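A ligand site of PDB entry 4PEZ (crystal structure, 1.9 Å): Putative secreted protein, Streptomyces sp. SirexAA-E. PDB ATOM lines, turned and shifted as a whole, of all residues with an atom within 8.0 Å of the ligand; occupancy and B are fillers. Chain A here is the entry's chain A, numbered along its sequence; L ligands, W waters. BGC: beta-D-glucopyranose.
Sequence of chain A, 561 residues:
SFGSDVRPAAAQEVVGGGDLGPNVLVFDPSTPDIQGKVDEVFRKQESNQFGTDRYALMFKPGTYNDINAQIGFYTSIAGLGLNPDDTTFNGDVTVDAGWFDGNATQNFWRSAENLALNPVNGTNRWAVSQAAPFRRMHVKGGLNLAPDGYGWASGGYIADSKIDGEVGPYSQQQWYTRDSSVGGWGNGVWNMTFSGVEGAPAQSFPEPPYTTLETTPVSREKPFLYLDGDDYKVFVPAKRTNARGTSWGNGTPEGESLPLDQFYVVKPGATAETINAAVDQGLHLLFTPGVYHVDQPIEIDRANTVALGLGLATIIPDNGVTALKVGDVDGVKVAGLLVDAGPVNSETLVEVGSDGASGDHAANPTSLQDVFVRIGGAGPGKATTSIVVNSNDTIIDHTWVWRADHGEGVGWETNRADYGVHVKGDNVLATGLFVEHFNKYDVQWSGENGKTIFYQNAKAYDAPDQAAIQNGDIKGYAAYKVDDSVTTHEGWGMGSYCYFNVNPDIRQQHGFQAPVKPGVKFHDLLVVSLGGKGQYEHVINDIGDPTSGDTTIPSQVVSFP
NH1 of Arg 125 lies within hydrogen-bond range of O2 of the ligand, at 2.5 Å. O5 of the ligand lies within hydrogen-bond range of ND2 of Asn 68 (3.1 Å). ND2 of Asn 121 is in hydrogen-bond range of O4 of the ligand, at 3.4 Å.
NE of Arg 125 is in hydrogen-bond range of O of Ala 146 (3.1 Å). The side-chain hydroxyl of Thr 94 sits at hydrogen-bond distance from the side-chain amide oxygen of Asn 68 (2.7 Å). The side-chain amide oxygen (OD1) of Asn 121 sits at hydrogen-bond distance from the backbone NH (N) of Thr 123, 2.9 Å away. The side-chain carboxylate (OD1) of Asp 92 lies within hydrogen-bond range of the backbone NH (N) of Val 120. N of Thr 94 lies within hydrogen-bond range of O of Ala 69. O of Ile 67 sits at hydrogen-bond distance from N of Asp 92 (2.9 Å). N of Ala 69 is in hydrogen-bond range of O of Asp 92 (2.9 Å). N of Asp 148 sits at hydrogen-bond distance from OD1 of Asp 96 (3.1 Å).
Asp 92 touches the ligand (OD2 to C4, 3.7 Å). Thr 94 touches the ligand. Asp 96 touches the ligand (OD2 to O2, 3.9 Å). Val 120 touches the ligand (CG1 to C6, 3.5 Å). Thr 123 touches the ligand. Hydrophobic or aromatic side chains within 4 Å of the ligand: Val 120. Of the 24 residues printed, 8 come within 4 Å of the ligand. Along chain A the residues within 4 Å of the ligand span positions 68 to 125. The nearest printed residue that does not touch the ligand is Asn 124 (4.7 Å).
Water W3 lies within hydrogen-bond range of an oxygen (O3) of the ligand (2.6 Å), the side-chain carboxylate of Asp 92 (2.8 Å), the side-chain hydroxyl of Thr 94 (2.8 Å) and the backbone NH of Arg 125 (2.9 Å). Water W4 lies within hydrogen-bond range of O3 of the ligand, O of Thr 123 and ND2 of Asn 121.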
ATOM      1  N   ILE A  67       7.896 -19.689   1.179  1.00  0.00           N
ATOM      2  CA  ILE A  67       7.546 -18.571   2.036  1.00  0.00           C
ATOM      3  C   ILE A  67       8.666 -18.301   3.034  1.00  0.00           C
ATOM      4  O   ILE A  67       9.191 -19.210   3.675  1.00  0.00           O
ATOM      5  CB  ILE A  67       6.210 -18.821   2.774  1.00  0.00           C
ATOM      6  CG1 ILE A  67       5.846 -17.609   3.627  1.00  0.00           C
ATOM      7  CG2 ILE A  67       6.230 -20.130   3.588  1.00  0.00           C
ATOM      8  CD1 ILE A  67       4.477 -17.722   4.264  1.00  0.00           C
ATOM      9  N   ASN A  68       9.075 -17.045   3.110  1.00  0.00           N
ATOM     10  CA  ASN A  68       9.937 -16.579   4.181  1.00  0.00           C
ATOM     11  C   ASN A  68       9.266 -15.388   4.855  1.00  0.00           C
ATOM     12  O   ASN A  68       9.348 -14.264   4.361  1.00  0.00           O
ATOM     13  CB  ASN A  68      11.327 -16.194   3.658  1.00  0.00           C
ATOM     14  CG  ASN A  68      12.259 -15.758   4.769  1.00  0.00           C
ATOM     15  OD1 ASN A  68      12.032 -16.049   5.953  1.00  0.00           O
ATOM     16  ND2 ASN A  68      13.324 -15.057   4.400  1.00  0.00           N
ATOM     17  N   ALA A  69       8.565 -15.651   5.948  1.00  0.00           N
ATOM     18  CA  ALA A  69       7.825 -14.607   6.659  1.00  0.00           C
ATOM     19  C   ALA A  69       8.775 -13.876   7.605  1.00  0.00           C
ATOM     20  O   ALA A  69       9.086 -14.370   8.700  1.00  0.00           O
ATOM     21  CB  ALA A  69       6.634 -15.212   7.402  1.00  0.00           C
ATOM     22  N   GLN A  70       9.261 -12.713   7.185  1.00  0.00           N
ATOM     23  CA  GLN A  70      10.120 -11.912   8.052  1.00  0.00           C
ATOM     24  C   GLN A  70       9.265 -11.059   8.976  1.00  0.00           C
ATOM     25  O   GLN A  70       8.361 -10.362   8.529  1.00  0.00           O
ATOM     26  CB  GLN A  70      11.068 -11.037   7.223  1.00  0.00           C
ATOM     27  CG  GLN A  70      12.160 -11.815   6.509  1.00  0.00           C
ATOM     28  CD  GLN A  70      13.132 -10.915   5.770  1.00  0.00           C
ATOM     29  OE1 GLN A  70      14.068 -10.356   6.367  1.00  0.00           O
ATOM     30  NE2 GLN A  70      12.905 -10.747   4.468  1.00  0.00           N
ATOM     31  N   GLY A  91       9.308 -23.490   4.412  1.00  0.00           N
ATOM     32  CA  GLY A  91       9.803 -22.136   4.514  1.00  0.00           C
ATOM     33  C   GLY A  91      10.007 -21.733   5.967  1.00  0.00           C
ATOM     34  O   GLY A  91      10.111 -22.578   6.858  1.00  0.00           O
ATOM     35  N   ASP A  92      10.065 -20.434   6.192  1.00  0.00           N
ATOM     36  CA  ASP A  92      10.576 -19.913   7.454  1.00  0.00           C
ATOM     37  C   ASP A  92       9.703 -18.830   8.076  1.00  0.00           C
ATOM     38  O   ASP A  92       8.936 -18.158   7.381  1.00  0.00           O
ATOM     39  CB  ASP A  92      11.984 -19.345   7.258  1.00  0.00           C
ATOM     40  CG  ASP A  92      12.999 -20.383   6.774  1.00  0.00           C
ATOM     41  OD1 ASP A  92      12.750 -21.056   5.753  1.00  0.00           O
ATOM     42  OD2 ASP A  92      14.078 -20.506   7.410  1.00  0.00           O
ATOM     43  N   VAL A  93       9.842 -18.676   9.386  1.00  0.00           N
ATOM     44  CA  VAL A  93       9.358 -17.508  10.105  1.00  0.00           C
ATOM     45  C   VAL A  93      10.602 -16.892  10.753  1.00  0.00           C
ATOM     46  O   VAL A  93      11.175 -17.447  11.698  1.00  0.00           O
ATOM     47  CB  VAL A  93       8.304 -17.877  11.167  1.00  0.00           C
ATOM     48  CG1 VAL A  93       8.001 -16.669  12.062  1.00  0.00           C
ATOM     49  CG2 VAL A  93       7.031 -18.367  10.496  1.00  0.00           C
ATOM     50  N   THR A  94      11.043 -15.775  10.189  1.00  0.00           N
ATOM     51  CA  THR A  94      12.390 -15.269  10.415  1.00  0.00           C
ATOM     52  C   THR A  94      12.419 -13.937  11.158  1.00  0.00           C
ATOM     53  O   THR A  94      11.731 -12.990  10.776  1.00  0.00           O
ATOM     54  CB  THR A  94      13.144 -15.062   9.071  1.00  0.00           C
ATOM     55  OG1 THR A  94      13.172 -16.284   8.336  1.00  0.00           O
ATOM     56  CG2 THR A  94      14.574 -14.565   9.322  1.00  0.00           C
ATOM     57  N   VAL A  95      13.226 -13.876  12.211  1.00  0.00           N
ATOM     58  CA  VAL A  95      13.648 -12.591  12.779  1.00  0.00           C
ATOM     59  C   VAL A  95      15.172 -12.493  12.699  1.00  0.00           C
ATOM     60  O   VAL A  95      15.884 -13.396  13.143  1.00  0.00           O
ATOM     61  CB  VAL A  95      13.196 -12.422  14.227  1.00  0.00           C
ATOM     62  CG1 VAL A  95      13.720 -11.093  14.802  1.00  0.00           C
ATOM     63  CG2 VAL A  95      11.673 -12.460  14.322  1.00  0.00           C
ATOM     64  N   ASP A  96      15.664 -11.401  12.127  1.00  0.00           N
ATOM     65  CA  ASP A  96      17.105 -11.167  12.045  1.00  0.00           C
ATOM     66  C   ASP A  96      17.338  -9.701  12.440  1.00  0.00           C
ATOM     67  O   ASP A  96      16.391  -8.990  12.755  1.00  0.00           O
ATOM     68  CB  ASP A  96      17.628 -11.480  10.643  1.00  0.00           C
ATOM     69  CG  ASP A  96      19.142 -11.772  10.597  1.00  0.00           C
ATOM     70  OD1 ASP A  96      19.855 -11.562  11.607  1.00  0.00           O
ATOM     71  OD2 ASP A  96      19.608 -12.216   9.529  1.00  0.00           O
ATOM     72  N   ALA A  97      18.592  -9.261  12.422  1.00  0.00           N
ATOM     73  CA  ALA A  97      18.919  -7.941  12.953  1.00  0.00           C
ATOM     74  C   ALA A  97      19.533  -6.996  11.913  1.00  0.00           C
ATOM     75  O   ALA A  97      20.316  -6.117  12.263  1.00  0.00           O
ATOM     76  CB  ALA A  97      19.877  -8.089  14.140  1.00  0.00           C
ATOM     77  N   PRO A 119      12.106 -25.447   7.572  1.00  0.00           N
ATOM     78  CA  PRO A 119      12.916 -24.299   7.122  1.00  0.00           C
ATOM     79  C   PRO A 119      13.759 -24.655   5.903  1.00  0.00           C
ATOM     80  O   PRO A 119      14.242 -25.770   5.813  1.00  0.00           O
ATOM     81  CB  PRO A 119      13.804 -23.968   8.330  1.00  0.00           C
ATOM     82  CG  PRO A 119      13.813 -25.208   9.174  1.00  0.00           C
ATOM     83  CD  PRO A 119      12.497 -25.920   8.921  1.00  0.00           C
ATOM     84  N   VAL A 120      13.924 -23.696   5.004  1.00  0.00           N
ATOM     85  CA  VAL A 120      14.461 -23.962   3.686  1.00  0.00           C
ATOM     86  C   VAL A 120      15.919 -24.459   3.688  1.00  0.00           C
ATOM     87  O   VAL A 120      16.289 -25.260   2.824  1.00  0.00           O
ATOM     88  CB  VAL A 120      14.305 -22.698   2.777  1.00  0.00           C
ATOM     89  CG1 VAL A 120      15.125 -21.537   3.317  1.00  0.00           C
ATOM     90  CG2 VAL A 120      14.684 -23.016   1.337  1.00  0.00           C
ATOM     91  N   ASN A 121      16.752 -24.019   4.627  1.00  0.00           N
ATOM     92  CA  ASN A 121      18.096 -24.585   4.709  1.00  0.00           C
ATOM     93  C   ASN A 121      18.241 -25.553   5.879  1.00  0.00           C
ATOM     94  O   ASN A 121      19.353 -25.913   6.259  1.00  0.00           O
ATOM     95  CB  ASN A 121      19.172 -23.475   4.763  1.00  0.00           C
ATOM     96  CG  ASN A 121      19.238 -22.746   6.103  1.00  0.00           C
ATOM     97  OD1 ASN A 121      18.596 -23.117   7.101  1.00  0.00           O
ATOM     98  ND2 ASN A 121      20.035 -21.676   6.138  1.00  0.00           N
ATOM     99  N   GLY A 122      17.121 -25.948   6.465  1.00  0.00           N
ATOM    100  CA  GLY A 122      17.130 -26.887   7.583  1.00  0.00           C
ATOM    101  C   GLY A 122      17.148 -26.245   8.964  1.00  0.00           C
ATOM    102  O   GLY A 122      16.953 -26.943   9.962  1.00  0.00           O
ATOM    103  N   THR A 123      17.386 -24.938   9.028  1.00  0.00           N
ATOM    104  CA  THR A 123      17.410 -24.205  10.302  1.00  0.00           C
ATOM    105  C   THR A 123      16.610 -22.911  10.224  1.00  0.00           C
ATOM    106  O   THR A 123      16.813 -22.110   9.325  1.00  0.00           O
ATOM    107  CB  THR A 123      18.865 -23.860  10.719  1.00  0.00           C
ATOM    108  OG1 THR A 123      19.615 -25.060  10.934  1.00  0.00           O
ATOM    109  CG2 THR A 123      18.874 -23.051  12.017  1.00  0.00           C
ATOM    110  N   ASN A 124      15.677 -22.729  11.160  1.00  0.00           N
ATOM    111  CA  ASN A 124      14.929 -21.485  11.246  1.00  0.00           C
ATOM    112  C   ASN A 124      15.651 -20.480  12.148  1.00  0.00           C
ATOM    113  O   ASN A 124      16.212 -20.856  13.188  1.00  0.00           O
ATOM    114  CB  ASN A 124      13.515 -21.738  11.795  1.00  0.00           C
ATOM    115  CG  ASN A 124      12.576 -20.573  11.520  1.00  0.00           C
ATOM    116  OD1 ASN A 124      12.038 -20.449  10.424  1.00  0.00           O
ATOM    117  ND2 ASN A 124      12.386 -19.714  12.517  1.00  0.00           N
ATOM    118  N   ARG A 125      15.647 -19.206  11.760  1.00  0.00           N
ATOM    119  CA  ARG A 125      16.263 -18.168  12.598  1.00  0.00           C
ATOM    120  C   ARG A 125      15.231 -17.269  13.297  1.00  0.00           C
ATOM    121  O   ARG A 125      14.458 -16.564  12.639  1.00  0.00           O
ATOM    122  CB  ARG A 125      17.213 -17.294  11.783  1.00  0.00           C
ATOM    123  CG  ARG A 125      17.924 -16.245  12.644  1.00  0.00           C
ATOM    124  CD  ARG A 125      18.794 -15.295  11.841  1.00  0.00           C
ATOM    125  NE  ARG A 125      20.158 -15.802  11.670  1.00  0.00           N
ATOM    126  CZ  ARG A 125      20.621 -16.318  10.546  1.00  0.00           C
ATOM    127  NH1 ARG A 125      19.835 -16.409   9.482  1.00  0.00           N
ATOM    128  NH2 ARG A 125      21.872 -16.751  10.463  1.00  0.00           N
ATOM    129  N   TRP A 126      15.264 -17.284  14.628  1.00  0.00           N
ATOM    130  CA  TRP A 126      14.397 -16.454  15.475  1.00  0.00           C
ATOM    131  C   TRP A 126      15.298 -15.626  16.408  1.00  0.00           C
ATOM    132  O   TRP A 126      15.450 -15.950  17.590  1.00  0.00           O
ATOM    133  CB  TRP A 126      13.434 -17.361  16.263  1.00  0.00           C
ATOM    134  CG  TRP A 126      12.345 -16.671  17.068  1.00  0.00           C
ATOM    135  CD1 TRP A 126      12.258 -16.588  18.423  1.00  0.00           C
ATOM    136  CD2 TRP A 126      11.177 -16.014  16.549  1.00  0.00           C
ATOM    137  NE1 TRP A 126      11.116 -15.913  18.786  1.00  0.00           N
ATOM    138  CE2 TRP A 126      10.437 -15.545  17.647  1.00  0.00           C
ATOM    139  CE3 TRP A 126      10.693 -15.761  15.255  1.00  0.00           C
ATOM    140  CZ2 TRP A 126       9.236 -14.839  17.498  1.00  0.00           C
ATOM    141  CZ3 TRP A 126       9.500 -15.075  15.111  1.00  0.00           C
ATOM    142  CH2 TRP A 126       8.785 -14.612  16.220  1.00  0.00           C
ATOM    143  N   ALA A 127      15.938 -14.603  15.858  1.00  0.00           N
ATOM    144  CA  ALA A 127      16.979 -13.877  16.585  1.00  0.00           C
ATOM    145  C   ALA A 127      16.383 -12.691  17.320  1.00  0.00           C
ATOM    146  O   ALA A 127      16.427 -11.545  16.853  1.00  0.00           O
ATOM    147  CB  ALA A 127      18.085 -13.429  15.652  1.00  0.00           C
ATOM    148  N   ASN A 144      17.909 -21.458  15.155  1.00  0.00           N
ATOM    149  CA  ASN A 144      19.033 -20.563  15.451  1.00  0.00           C
ATOM    150  C   ASN A 144      18.502 -19.312  16.128  1.00  0.00           C
ATOM    151  O   ASN A 144      17.716 -18.584  15.528  1.00  0.00           O
ATOM    152  CB  ASN A 144      19.781 -20.209  14.152  1.00  0.00           C
ATOM    153  CG  ASN A 144      21.053 -19.385  14.392  1.00  0.00           C
ATOM    154  OD1 ASN A 144      21.209 -18.740  15.432  1.00  0.00           O
ATOM    155  ND2 ASN A 144      21.952 -19.403  13.412  1.00  0.00           N
ATOM    156  N   ALA A 146      20.369 -16.717  17.186  1.00  0.00           N
ATOM    157  CA  ALA A 146      21.311 -15.606  17.052  1.00  0.00           C
ATOM    158  C   ALA A 146      21.173 -14.890  15.700  1.00  0.00           C
ATOM    159  O   ALA A 146      20.820 -15.511  14.694  1.00  0.00           O
ATOM    160  CB  ALA A 146      22.763 -16.108  17.234  1.00  0.00           C
ATOM    161  N   PRO A 147      21.440 -13.575  15.683  1.00  0.00           N
ATOM    162  CA  PRO A 147      21.467 -12.804  14.437  1.00  0.00           C
ATOM    163  C   PRO A 147      22.586 -13.296  13.529  1.00  0.00           C
ATOM    164  O   PRO A 147      23.561 -13.886  14.004  1.00  0.00           O
ATOM    165  CB  PRO A 147      21.740 -11.358  14.912  1.00  0.00           C
ATOM    166  CG  PRO A 147      22.370 -11.499  16.244  1.00  0.00           C
ATOM    167  CD  PRO A 147      21.744 -12.733  16.862  1.00  0.00           C
ATOM    168  N   ASP A 148      22.454 -13.064  12.229  1.00  0.00           N
ATOM    169  CA  ASP A 148      23.503 -13.436  11.296  1.00  0.00           C
ATOM    170  C   ASP A 148      24.740 -12.600  11.626  1.00  0.00           C
ATOM    171  O   ASP A 148      24.683 -11.367  11.616  1.00  0.00           O
ATOM    172  CB  ASP A 148      23.051 -13.207   9.854  1.00  0.00           C
ATOM    173  CG  ASP A 148      24.099 -13.606   8.836  1.00  0.00           C
ATOM    174  OD1 ASP A 148      24.955 -14.449   9.160  1.00  0.00           O
ATOM    175  OD2 ASP A 148      24.063 -13.084   7.703  1.00  0.00           O
HETATM  176  C2  BGC L   1      16.996 -16.177   7.276  1.00  0.00           C
HETATM  177  C3  BGC L   1      17.460 -17.618   7.092  1.00  0.00           C
HETATM  178  C4  BGC L   1      16.744 -18.326   5.942  1.00  0.00           C
HETATM  179  C5  BGC L   1      16.685 -17.437   4.709  1.00  0.00           C
HETATM  180  C6  BGC L   1      15.906 -18.134   3.604  1.00  0.00           C
HETATM  181  C1  BGC L   1      16.864 -15.444   5.938  1.00  0.00           C
HETATM  182  O2  BGC L   1      17.898 -15.472   8.115  1.00  0.00           O
HETATM  183  O3  BGC L   1      17.256 -18.338   8.285  1.00  0.00           O
HETATM  184  O4  BGC L   1      17.417 -19.522   5.597  1.00  0.00           O
HETATM  185  O5  BGC L   1      16.077 -16.217   5.047  1.00  0.00           O
HETATM  186  O6  BGC L   1      15.941 -17.363   2.414  1.00  0.00           O
HETATM  187  O   HOH W   1      13.556 -18.766   1.330  1.00  0.00           O
HETATM  188  O   HOH W   2      16.256 -21.652   6.537  1.00  0.00           O
HETATM  189  O   HOH W   3      14.803 -18.447   9.120  1.00  0.00           O
HETATM  190  O   HOH W   4      19.125 -20.303   8.995  1.00  0.00           O
